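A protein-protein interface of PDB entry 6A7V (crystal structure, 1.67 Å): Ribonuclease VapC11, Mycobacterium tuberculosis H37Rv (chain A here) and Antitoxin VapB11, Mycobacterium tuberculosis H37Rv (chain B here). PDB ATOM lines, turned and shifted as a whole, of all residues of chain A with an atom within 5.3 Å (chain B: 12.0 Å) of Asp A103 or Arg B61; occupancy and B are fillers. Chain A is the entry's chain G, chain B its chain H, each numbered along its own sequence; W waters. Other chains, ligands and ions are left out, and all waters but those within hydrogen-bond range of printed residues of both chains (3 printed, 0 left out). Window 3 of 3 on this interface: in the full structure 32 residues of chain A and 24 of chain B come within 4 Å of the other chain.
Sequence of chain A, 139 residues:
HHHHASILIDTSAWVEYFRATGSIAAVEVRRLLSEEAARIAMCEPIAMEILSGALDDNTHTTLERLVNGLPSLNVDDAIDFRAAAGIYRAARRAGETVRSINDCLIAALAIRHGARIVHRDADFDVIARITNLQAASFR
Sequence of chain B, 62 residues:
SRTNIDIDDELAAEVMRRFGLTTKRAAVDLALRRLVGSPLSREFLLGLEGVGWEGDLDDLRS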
ATOM      1  N   ASP A  10      23.231 -12.744   4.448  1.00  0.00           N
ATOM      2  CA  ASP A  10      23.744 -13.475   3.292  1.00  0.00           C
ATOM      3  C   ASP A  10      22.662 -13.628   2.232  1.00  0.00           C
ATOM      4  O   ASP A  10      21.469 -13.568   2.530  1.00  0.00           O
ATOM      5  CB  ASP A  10      24.242 -14.859   3.704  1.00  0.00           C
ATOM      6  CG  ASP A  10      24.928 -15.596   2.564  1.00  0.00           C
ATOM      7  OD1 ASP A  10      25.870 -15.027   1.966  1.00  0.00           O
ATOM      8  OD2 ASP A  10      24.525 -16.742   2.255  1.00  0.00           O
ATOM      9  N   THR A  11      23.101 -13.842   0.996  1.00  0.00           N
ATOM     10  CA  THR A  11      22.210 -14.072  -0.126  1.00  0.00           C
ATOM     11  C   THR A  11      21.245 -15.215   0.153  1.00  0.00           C
ATOM     12  O   THR A  11      20.095 -15.118  -0.237  1.00  0.00           O
ATOM     13  CB  THR A  11      23.008 -14.396  -1.393  1.00  0.00           C
ATOM     14  OG1 THR A  11      24.053 -13.433  -1.544  1.00  0.00           O
ATOM     15  CG2 THR A  11      22.112 -14.361  -2.617  1.00  0.00           C
ATOM     16  N   SER A  12      21.725 -16.209   0.892  1.00  0.00           N
ATOM     17  CA  SER A  12      20.947 -17.418   1.160  1.00  0.00           C
ATOM     18  C   SER A  12      19.668 -17.099   1.941  1.00  0.00           C
ATOM     19  O   SER A  12      18.606 -17.574   1.588  1.00  0.00           O
ATOM     20  CB  SER A  12      21.804 -18.457   1.893  1.00  0.00           C
ATOM     21  OG  SER A  12      22.292 -17.951   3.124  1.00  0.00           O
ATOM     22  N   ILE A  46      27.622  -9.981  -2.314  1.00  0.00           N
ATOM     23  CA  ILE A  46      26.236 -10.353  -2.081  1.00  0.00           C
ATOM     24  C   ILE A  46      25.298  -9.677  -3.093  1.00  0.00           C
ATOM     25  O   ILE A  46      24.404 -10.299  -3.638  1.00  0.00           O
ATOM     26  CB  ILE A  46      25.799 -10.066  -0.620  1.00  0.00           C
ATOM     27  CG1 ILE A  46      26.501 -11.055   0.325  1.00  0.00           C
ATOM     28  CG2 ILE A  46      24.284 -10.181  -0.466  1.00  0.00           C
ATOM     29  CD1 ILE A  46      26.302 -10.780   1.808  1.00  0.00           C
ATOM     30  N   GLU A  49      25.395 -11.250  -6.470  1.00  0.00           N
ATOM     31  CA  GLU A  49      24.642 -12.487  -6.448  1.00  0.00           C
ATOM     32  C   GLU A  49      23.126 -12.204  -6.584  1.00  0.00           C
ATOM     33  O   GLU A  49      22.396 -12.781  -7.384  1.00  0.00           O
ATOM     34  CB  GLU A  49      24.933 -13.313  -5.198  1.00  0.00           C
ATOM     35  CG  GLU A  49      26.325 -13.939  -5.204  1.00  0.00           C
ATOM     36  CD  GLU A  49      26.585 -14.813  -3.994  1.00  0.00           C
ATOM     37  OE1 GLU A  49      26.053 -14.510  -2.906  1.00  0.00           O
ATOM     38  OE2 GLU A  49      27.329 -15.805  -4.123  1.00  0.00           O
ATOM     39  N   ARG A  99      31.360 -24.959  -0.806  1.00  0.00           N
ATOM     40  CA  ARG A  99      30.674 -24.929  -2.096  1.00  0.00           C
ATOM     41  C   ARG A  99      30.946 -23.660  -2.918  1.00  0.00           C
ATOM     42  O   ARG A  99      30.970 -23.732  -4.142  1.00  0.00           O
ATOM     43  CB  ARG A  99      29.168 -25.182  -1.929  1.00  0.00           C
ATOM     44  CG  ARG A  99      28.384 -24.080  -1.238  1.00  0.00           C
ATOM     45  CD  ARG A  99      27.102 -24.612  -0.606  1.00  0.00           C
ATOM     46  NE  ARG A  99      26.055 -24.837  -1.602  1.00  0.00           N
ATOM     47  CZ  ARG A  99      25.297 -23.882  -2.139  1.00  0.00           C
ATOM     48  NH1 ARG A  99      24.373 -24.201  -3.039  1.00  0.00           N
ATOM     49  NH2 ARG A  99      25.453 -22.607  -1.789  1.00  0.00           N
ATOM     50  N   SER A 100      31.168 -22.517  -2.264  1.00  0.00           N
ATOM     51  CA  SER A 100      31.440 -21.261  -2.982  1.00  0.00           C
ATOM     52  C   SER A 100      32.617 -20.483  -2.384  1.00  0.00           C
ATOM     53  O   SER A 100      32.580 -20.101  -1.222  1.00  0.00           O
ATOM     54  CB  SER A 100      30.194 -20.373  -2.981  1.00  0.00           C
ATOM     55  OG  SER A 100      30.417 -19.152  -3.674  1.00  0.00           O
ATOM     56  N   ILE A 101      33.648 -20.243  -3.188  1.00  0.00           N
ATOM     57  CA  ILE A 101      34.756 -19.420  -2.797  1.00  0.00           C
ATOM     58  C   ILE A 101      34.341 -17.992  -2.516  1.00  0.00           C
ATOM     59  O   ILE A 101      34.993 -17.364  -1.696  1.00  0.00           O
ATOM     60  CB  ILE A 101      35.905 -19.495  -3.825  1.00  0.00           C
ATOM     61  CG1 ILE A 101      37.200 -18.978  -3.192  1.00  0.00           C
ATOM     62  CG2 ILE A 101      35.544 -18.749  -5.104  1.00  0.00           C
ATOM     63  CD1 ILE A 101      38.443 -19.540  -3.830  1.00  0.00           C
ATOM     64  N   ASN A 102      33.228 -17.524  -3.069  1.00  0.00           N
ATOM     65  CA  ASN A 102      32.709 -16.212  -2.719  1.00  0.00           C
ATOM     66  C   ASN A 102      32.127 -16.183  -1.327  1.00  0.00           C
ATOM     67  O   ASN A 102      32.242 -15.133  -0.717  1.00  0.00           O
ATOM     68  CB  ASN A 102      31.741 -15.686  -3.776  1.00  0.00           C
ATOM     69  CG  ASN A 102      32.467 -15.121  -4.978  1.00  0.00           C
ATOM     70  OD1 ASN A 102      33.677 -14.860  -4.923  1.00  0.00           O
ATOM     71  ND2 ASN A 102      31.743 -14.928  -6.071  1.00  0.00           N
ATOM     72  N   ASP A 103      31.735 -17.301  -0.737  1.00  0.00           N
ATOM     73  CA  ASP A 103      31.405 -17.311   0.682  1.00  0.00           C
ATOM     74  C   ASP A 103      32.637 -17.082   1.544  1.00  0.00           C
ATOM     75  O   ASP A 103      32.561 -16.373   2.521  1.00  0.00           O
ATOM     76  CB  ASP A 103      30.691 -18.601   1.072  1.00  0.00           C
ATOM     77  CG  ASP A 103      29.300 -18.685   0.473  1.00  0.00           C
ATOM     78  OD1 ASP A 103      28.787 -17.627   0.053  1.00  0.00           O
ATOM     79  OD2 ASP A 103      28.720 -19.789   0.414  1.00  0.00           O
ATOM     80  N   CYS A 104      33.773 -17.570   1.121  1.00  0.00           N
ATOM     81  CA  CYS A 104      35.024 -17.271   1.844  1.00  0.00           C
ATOM     82  C   CYS A 104      35.353 -15.799   1.723  1.00  0.00           C
ATOM     83  O   CYS A 104      35.733 -15.192   2.734  1.00  0.00           O
ATOM     84  CB  CYS A 104      36.205 -18.085   1.303  1.00  0.00           C
ATOM     85  SG  CYS A 104      36.054 -19.861   1.554  1.00  0.00           S
ATOM     86  N   LEU A 105      35.119 -15.184   0.601  1.00  0.00           N
ATOM     87  CA  LEU A 105      35.343 -13.766   0.405  1.00  0.00           C
ATOM     88  C   LEU A 105      34.440 -12.920   1.316  1.00  0.00           C
ATOM     89  O   LEU A 105      34.905 -11.995   2.000  1.00  0.00           O
ATOM     90  CB  LEU A 105      35.124 -13.344  -1.053  1.00  0.00           C
ATOM     91  CG  LEU A 105      35.322 -11.861  -1.404  1.00  0.00           C
ATOM     92  CD1 LEU A 105      36.749 -11.402  -1.162  1.00  0.00           C
ATOM     93  CD2 LEU A 105      34.949 -11.621  -2.864  1.00  0.00           C
ATOM     94  N   ILE A 106      33.178 -13.310   1.351  1.00  0.00           N
ATOM     95  CA  ILE A 106      32.180 -12.632   2.160  1.00  0.00           C
ATOM     96  C   ILE A 106      32.593 -12.726   3.642  1.00  0.00           C
ATOM     97  O   ILE A 106      32.524 -11.736   4.389  1.00  0.00           O
ATOM     98  CB  ILE A 106      30.755 -13.208   1.921  1.00  0.00           C
ATOM     99  CG1 ILE A 106      30.250 -12.824   0.521  1.00  0.00           C
ATOM    100  CG2 ILE A 106      29.771 -12.705   2.973  1.00  0.00           C
ATOM    101  CD1 ILE A 106      29.097 -13.668   0.012  1.00  0.00           C
ATOM    102  N   ALA A 107      32.977 -13.918   4.055  1.00  0.00           N
ATOM    103  CA  ALA A 107      33.379 -14.106   5.452  1.00  0.00           C
ATOM    104  C   ALA A 107      34.623 -13.307   5.781  1.00  0.00           C
ATOM    105  O   ALA A 107      34.668 -12.686   6.840  1.00  0.00           O
ATOM    106  CB  ALA A 107      33.619 -15.583   5.723  1.00  0.00           C
ATOM    107  N   ALA A 108      35.546 -13.232   4.854  1.00  0.00           N
ATOM    108  CA  ALA A 108      36.788 -12.498   4.997  1.00  0.00           C
ATOM    109  C   ALA A 108      36.459 -11.008   5.232  1.00  0.00           C
ATOM    110  O   ALA A 108      37.016 -10.346   6.115  1.00  0.00           O
ATOM    111  CB  ALA A 108      37.693 -12.678   3.788  1.00  0.00           C
ATOM    112  N   ASP A 121      23.532 -21.254   4.867  1.00  0.00           N
ATOM    113  CA  ASP A 121      24.469 -21.931   3.981  1.00  0.00           C
ATOM    114  C   ASP A 121      25.573 -22.543   4.852  1.00  0.00           C
ATOM    115  O   ASP A 121      26.221 -21.829   5.621  1.00  0.00           O
ATOM    116  CB  ASP A 121      25.036 -20.913   2.985  1.00  0.00           C
ATOM    117  CG  ASP A 121      25.749 -21.560   1.814  1.00  0.00           C
ATOM    118  OD1 ASP A 121      26.685 -22.351   2.048  1.00  0.00           O
ATOM    119  OD2 ASP A 121      25.391 -21.250   0.653  1.00  0.00           O
ATOM    120  N   ASP A 123      28.424 -23.324   4.317  1.00  0.00           N
ATOM    121  CA  ASP A 123      29.760 -22.767   4.129  1.00  0.00           C
ATOM    122  C   ASP A 123      30.117 -21.894   5.321  1.00  0.00           C
ATOM    123  O   ASP A 123      31.243 -21.960   5.837  1.00  0.00           O
ATOM    124  CB  ASP A 123      29.833 -21.877   2.883  1.00  0.00           C
ATOM    125  CG  ASP A 123      30.041 -22.660   1.599  1.00  0.00           C
ATOM    126  OD1 ASP A 123      30.101 -23.906   1.630  1.00  0.00           O
ATOM    127  OD2 ASP A 123      30.160 -22.006   0.543  1.00  0.00           O
ATOM    128  N   PHE A 124      29.182 -21.043   5.763  1.00  0.00           N
ATOM    129  CA  PHE A 124      29.420 -20.170   6.878  1.00  0.00           C
ATOM    130  C   PHE A 124      29.576 -20.908   8.178  1.00  0.00           C
ATOM    131  O   PHE A 124      30.379 -20.484   9.007  1.00  0.00           O
ATOM    132  CB  PHE A 124      28.368 -19.065   6.941  1.00  0.00           C
ATOM    133  CG  PHE A 124      28.414 -18.172   5.742  1.00  0.00           C
ATOM    134  CD1 PHE A 124      29.513 -17.361   5.526  1.00  0.00           C
ATOM    135  CD2 PHE A 124      27.403 -18.199   4.797  1.00  0.00           C
ATOM    136  CE1 PHE A 124      29.597 -16.559   4.400  1.00  0.00           C
ATOM    137  CE2 PHE A 124      27.475 -17.393   3.673  1.00  0.00           C
ATOM    138  CZ  PHE A 124      28.568 -16.572   3.476  1.00  0.00           C
ATOM    139  N   ILE A 127      33.113 -22.074   8.058  1.00  0.00           N
ATOM    140  CA  ILE A 127      34.059 -20.991   8.217  1.00  0.00           C
ATOM    141  C   ILE A 127      34.080 -20.574   9.687  1.00  0.00           C
ATOM    142  O   ILE A 127      35.184 -20.293  10.204  1.00  0.00           O
ATOM    143  CB  ILE A 127      33.794 -19.838   7.227  1.00  0.00           C
ATOM    144  CG1 ILE A 127      34.059 -20.321   5.790  1.00  0.00           C
ATOM    145  CG2 ILE A 127      34.693 -18.645   7.527  1.00  0.00           C
ATOM    146  CD1 ILE A 127      33.447 -19.454   4.711  1.00  0.00           C
ATOM    147  N   TRP B  53      12.356 -14.045  -6.614  1.00  0.00           N
ATOM    148  CA  TRP B  53      13.745 -14.189  -7.040  1.00  0.00           C
ATOM    149  C   TRP B  53      13.848 -15.489  -7.826  1.00  0.00           C
ATOM    150  O   TRP B  53      13.937 -16.568  -7.242  1.00  0.00           O
ATOM    151  CB  TRP B  53      14.676 -14.194  -5.825  1.00  0.00           C
ATOM    152  CG  TRP B  53      16.119 -13.943  -6.149  1.00  0.00           C
ATOM    153  CD1 TRP B  53      16.707 -12.735  -6.373  1.00  0.00           C
ATOM    154  CD2 TRP B  53      17.158 -14.922  -6.269  1.00  0.00           C
ATOM    155  NE1 TRP B  53      18.046 -12.900  -6.633  1.00  0.00           N
ATOM    156  CE2 TRP B  53      18.349 -14.232  -6.568  1.00  0.00           C
ATOM    157  CE3 TRP B  53      17.196 -16.315  -6.145  1.00  0.00           C
ATOM    158  CZ2 TRP B  53      19.572 -14.890  -6.749  1.00  0.00           C
ATOM    159  CZ3 TRP B  53      18.408 -16.968  -6.328  1.00  0.00           C
ATOM    160  CH2 TRP B  53      19.580 -16.254  -6.631  1.00  0.00           C
ATOM    161  N   GLY B  55      16.090 -16.572 -10.075  1.00  0.00           N
ATOM    162  CA  GLY B  55      17.399 -17.156 -10.338  1.00  0.00           C
ATOM    163  C   GLY B  55      17.625 -18.417  -9.532  1.00  0.00           C
ATOM    164  O   GLY B  55      16.787 -18.809  -8.715  1.00  0.00           O
ATOM    165  N   ASP B  56      18.764 -19.054  -9.771  1.00  0.00           N
ATOM    166  CA  ASP B  56      19.135 -20.275  -9.077  1.00  0.00           C
ATOM    167  C   ASP B  56      20.417 -20.003  -8.298  1.00  0.00           C
ATOM    168  O   ASP B  56      21.473 -19.801  -8.895  1.00  0.00           O
ATOM    169  CB  ASP B  56      19.340 -21.408 -10.092  1.00  0.00           C
ATOM    170  CG  ASP B  56      19.394 -22.787  -9.445  1.00  0.00           C
ATOM    171  OD1 ASP B  56      19.567 -22.879  -8.213  1.00  0.00           O
ATOM    172  OD2 ASP B  56      19.265 -23.789 -10.179  1.00  0.00           O
ATOM    173  N   LEU B  57      20.322 -19.985  -6.970  1.00  0.00           N
ATOM    174  CA  LEU B  57      21.491 -19.734  -6.119  1.00  0.00           C
ATOM    175  C   LEU B  57      22.530 -20.860  -6.217  1.00  0.00           C
ATOM    176  O   LEU B  57      23.722 -20.627  -5.997  1.00  0.00           O
ATOM    177  CB  LEU B  57      21.065 -19.524  -4.661  1.00  0.00           C
ATOM    178  CG  LEU B  57      22.147 -19.046  -3.687  1.00  0.00           C
ATOM    179  CD1 LEU B  57      22.771 -17.735  -4.146  1.00  0.00           C
ATOM    180  CD2 LEU B  57      21.571 -18.902  -2.287  1.00  0.00           C
ATOM    181  N   ASP B  58      22.078 -22.069  -6.553  1.00  0.00           N
ATOM    182  CA  ASP B  58      22.975 -23.201  -6.796  1.00  0.00           C
ATOM    183  C   ASP B  58      23.905 -22.957  -7.988  1.00  0.00           C
ATOM    184  O   ASP B  58      25.054 -23.389  -7.963  1.00  0.00           O
ATOM    185  CB  ASP B  58      22.183 -24.500  -7.017  1.00  0.00           C
ATOM    186  CG  ASP B  58      21.452 -24.971  -5.766  1.00  0.00           C
ATOM    187  OD1 ASP B  58      21.620 -24.353  -4.692  1.00  0.00           O
ATOM    188  OD2 ASP B  58      20.704 -25.969  -5.858  1.00  0.00           O
ATOM    189  N   ASP B  59      23.414 -22.280  -9.027  1.00  0.00           N
ATOM    190  CA  ASP B  59      24.260 -21.919 -10.175  1.00  0.00           C
ATOM    191  C   ASP B  59      25.359 -20.940  -9.776  1.00  0.00           C
ATOM    192  O   ASP B  59      26.501 -21.073 -10.209  1.00  0.00           O
ATOM    193  CB  ASP B  59      23.437 -21.299 -11.312  1.00  0.00           C
ATOM    194  CG  ASP B  59      22.624 -22.321 -12.083  1.00  0.00           C
ATOM    195  OD1 ASP B  59      22.998 -23.512 -12.096  1.00  0.00           O
ATOM    196  OD2 ASP B  59      21.610 -21.922 -12.691  1.00  0.00           O
ATOM    197  N   LEU B  60      25.000 -19.953  -8.957  1.00  0.00           N
ATOM    198  CA  LEU B  60      25.946 -18.927  -8.519  1.00  0.00           C
ATOM    199  C   LEU B  60      26.988 -19.484  -7.553  1.00  0.00           C
ATOM    200  O   LEU B  60      28.125 -19.023  -7.532  1.00  0.00           O
ATOM    201  CB  LEU B  60      25.201 -17.763  -7.859  1.00  0.00           C
ATOM    202  CG  LEU B  60      24.203 -17.007  -8.741  1.00  0.00           C
ATOM    203  CD1 LEU B  60      23.437 -15.989  -7.909  1.00  0.00           C
ATOM    204  CD2 LEU B  60      24.901 -16.332  -9.914  1.00  0.00           C
ATOM    205  N   ARG B  61      26.585 -20.473  -6.759  1.00  0.00           N
ATOM    206  CA  ARG B  61      27.445 -21.094  -5.753  1.00  0.00           C
ATOM    207  C   ARG B  61      27.759 -22.542  -6.156  1.00  0.00           C
ATOM    208  O   ARG B  61      28.788 -22.784  -6.783  1.00  0.00           O
ATOM    209  CB  ARG B  61      26.773 -20.984  -4.373  1.00  0.00           C
ATOM    210  CG  ARG B  61      26.595 -19.533  -3.946  1.00  0.00           C
ATOM    211  CD  ARG B  61      26.110 -19.369  -2.514  1.00  0.00           C
ATOM    212  NE  ARG B  61      26.158 -17.963  -2.110  1.00  0.00           N
ATOM    213  CZ  ARG B  61      25.864 -17.499  -0.896  1.00  0.00           C
ATOM    214  NH1 ARG B  61      25.486 -18.322   0.081  1.00  0.00           N
ATOM    215  NH2 ARG B  61      25.956 -16.195  -0.655  1.00  0.00           N
ATOM    216  N   SER B  62      26.886 -23.496  -5.825  1.00  0.00           N
ATOM    217  CA  SER B  62      27.057 -24.897  -6.256  1.00  0.00           C
ATOM    218  C   SER B  62      25.934 -25.797  -5.745  1.00  0.00           C
ATOM    219  O   SER B  62      25.837 -26.963  -6.135  1.00  0.00           O
ATOM    220  CB  SER B  62      28.414 -25.458  -5.813  1.00  0.00           C
ATOM    221  OG  SER B  62      29.398 -25.256  -6.812  1.00  0.00           O
HETATM  222  O   HOH W   1      32.021 -26.025  -5.608  1.00  0.00           O
HETATM  223  O   HOH W   2      29.086 -16.252  -5.927  1.00  0.00           O
HETATM  224  O   HOH W   3      29.040 -17.055  -2.560  1.00  0.00           O
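Among the printed residues, pairs that only touch across the chains: Thr A11 with Leu B57, Ser A12 with Leu B57, Glu A49 with Trp B53, Glu A49 with Leu B60, Arg A99 with Arg B61 and Ser A100 with Arg B61.
Water W2 lies within hydrogen-bond range of the side-chain carboxylate of Glu A49, the side-chain amide nitrogen of Asn A102 and the backbone carbonyl oxygen of Leu B60. Water W3 lies within hydrogen-bond range of OE2 of Glu A49 (2.6 Å), OD1 of Asp A103 (2.7 Å), OG of Ser A100 (2.7 Å) and NE of Arg B61 (3.1 Å). Water W1 bridges the backbone carbonyl oxygen (O) of Arg A99 (2.9 Å) and the side-chain hydroxyl (OG) of Ser B62 (3.0 Å).
Ser A12 touches just one residue of chain B: Leu B57 (3.8 Å). Of chain B, only Asp B58 (3.2 Å), Arg B61 (3.3 Å) and Ser B62 (3.5 Å) come within 4 Å of Arg A99. Ser A100 touches just one residue of chain B: Arg B61 (3.7 Å). Ile A101 touches none of the printed residues of chain B. No residue of chain B comes within 4 Å of Asn A102. Of chain B, only Arg B61 (3.1 Å) comes within 4 Å of Asp A103. No residue of chain B comes within 4 Å of Cys A104. No residue of chain B comes within 4 Å of Leu A105. No residue of chain B comes within 4 Å of Ile A106. No residue of chain B comes within 4 Å of Ala A107. Asp A121 touches just one residue of chain B: Arg B61. No residue of chain B comes within 4 Å of Asp A123. Of the printed residues of chain A, Leu B57 touches Thr A11 and Ser A12. Of the printed residues of chain A, Asp B58 touches Arg A99. Of the printed residues of chain A, Leu B60 touches Glu A49 (3.4 Å). Arg B61 touches just these residues of chain A: Asp A10 (2.9 Å), Thr A11 (3.5 Å), Glu A49 (2.8 Å), Arg A99 (3.3 Å), Ser A100 (3.7 Å), Asp A103 (3.1 Å) and Asp A121 (3.0 Å). The nearest printed residue of chain B that does not touch Glu A49 is Leu B57 (4.8 Å).
NH1 of Arg B61 lies within salt-bridge range of OD2 of Asp A10 (2.9 Å). The side-chain hydroxyl (OG1) of Thr A11 sits at hydrogen-bond distance from the guanidinium group (NH2) of Arg B61, 3.5 Å away. OE1 of Glu A49 lies within salt-bridge range of NH2 of Arg B61, 2.8 Å away. The side-chain carboxylate of Asp B58 is in salt-bridge range of the guanidinium group of Arg A99 (3.2 Å). The backbone carbonyl oxygen (O) of Arg A99 lies within hydrogen-bond range of the side-chain hydroxyl (OG) of Ser B62, at 3.5 Å. NH2 of Arg B61 lies within salt-bridge range of OD1 of Asp A103 (3.3 Å). NH1 of Arg B61 lies within salt-bridge range of OD2 of Asp A121.
The side-chain hydroxyl (OG1) of Thr A11 lies within hydrogen-bond range of the side-chain carboxylate (OE1) of Glu A49 (2.6 Å). NH2 of Arg A99 lies within salt-bridge range of OD2 of Asp A121 (2.8 Å). OD1 of Asp A123 lies within hydrogen-bond range of N of Arg A99 (2.9 Å). The backbone NH (N) of Ser A100 sits at hydrogen-bond distance from the side-chain carboxylate (OD2) of Asp A123 (3.0 Å). OD2 of Asp A103 sits close to OD2 of Asp A123 (2.6 Å). OD1 of Asp B56 sits at hydrogen-bond distance from N of Asp B58 (3.1 Å).
Printed residues of chain A that touch a printed residue of chain B: Asp A10, Thr A11, Ser A12, Glu A49, Arg A99, Ser A100, Asp A103 and Asp A121. Of the 9 printed residues of chain B, 6 touch a printed residue of chain A. Hydrophobic or aromatic side chains of chain B within 4 Å of the printed part of chain A: Trp B53, Leu B57 and Leu B60. Along chain B the printed residues that touch a printed residue of chain A span positions 53 to 62. Among the printed residues, 13 pairs touch across the chains. Among the printed residues, Asp or Glu carboxylates within 4 Å of a Lys or Arg side-chain nitrogen of the other chain: Asp A10 with Arg B61 (2.9 Å), Glu A49 with Arg B61 (2.8 Å), Arg A99 with Asp B58 (3.2 Å), Asp A103 with Arg B61 (3.3 Å) and Asp A121 with Arg B61 (3.0 Å).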
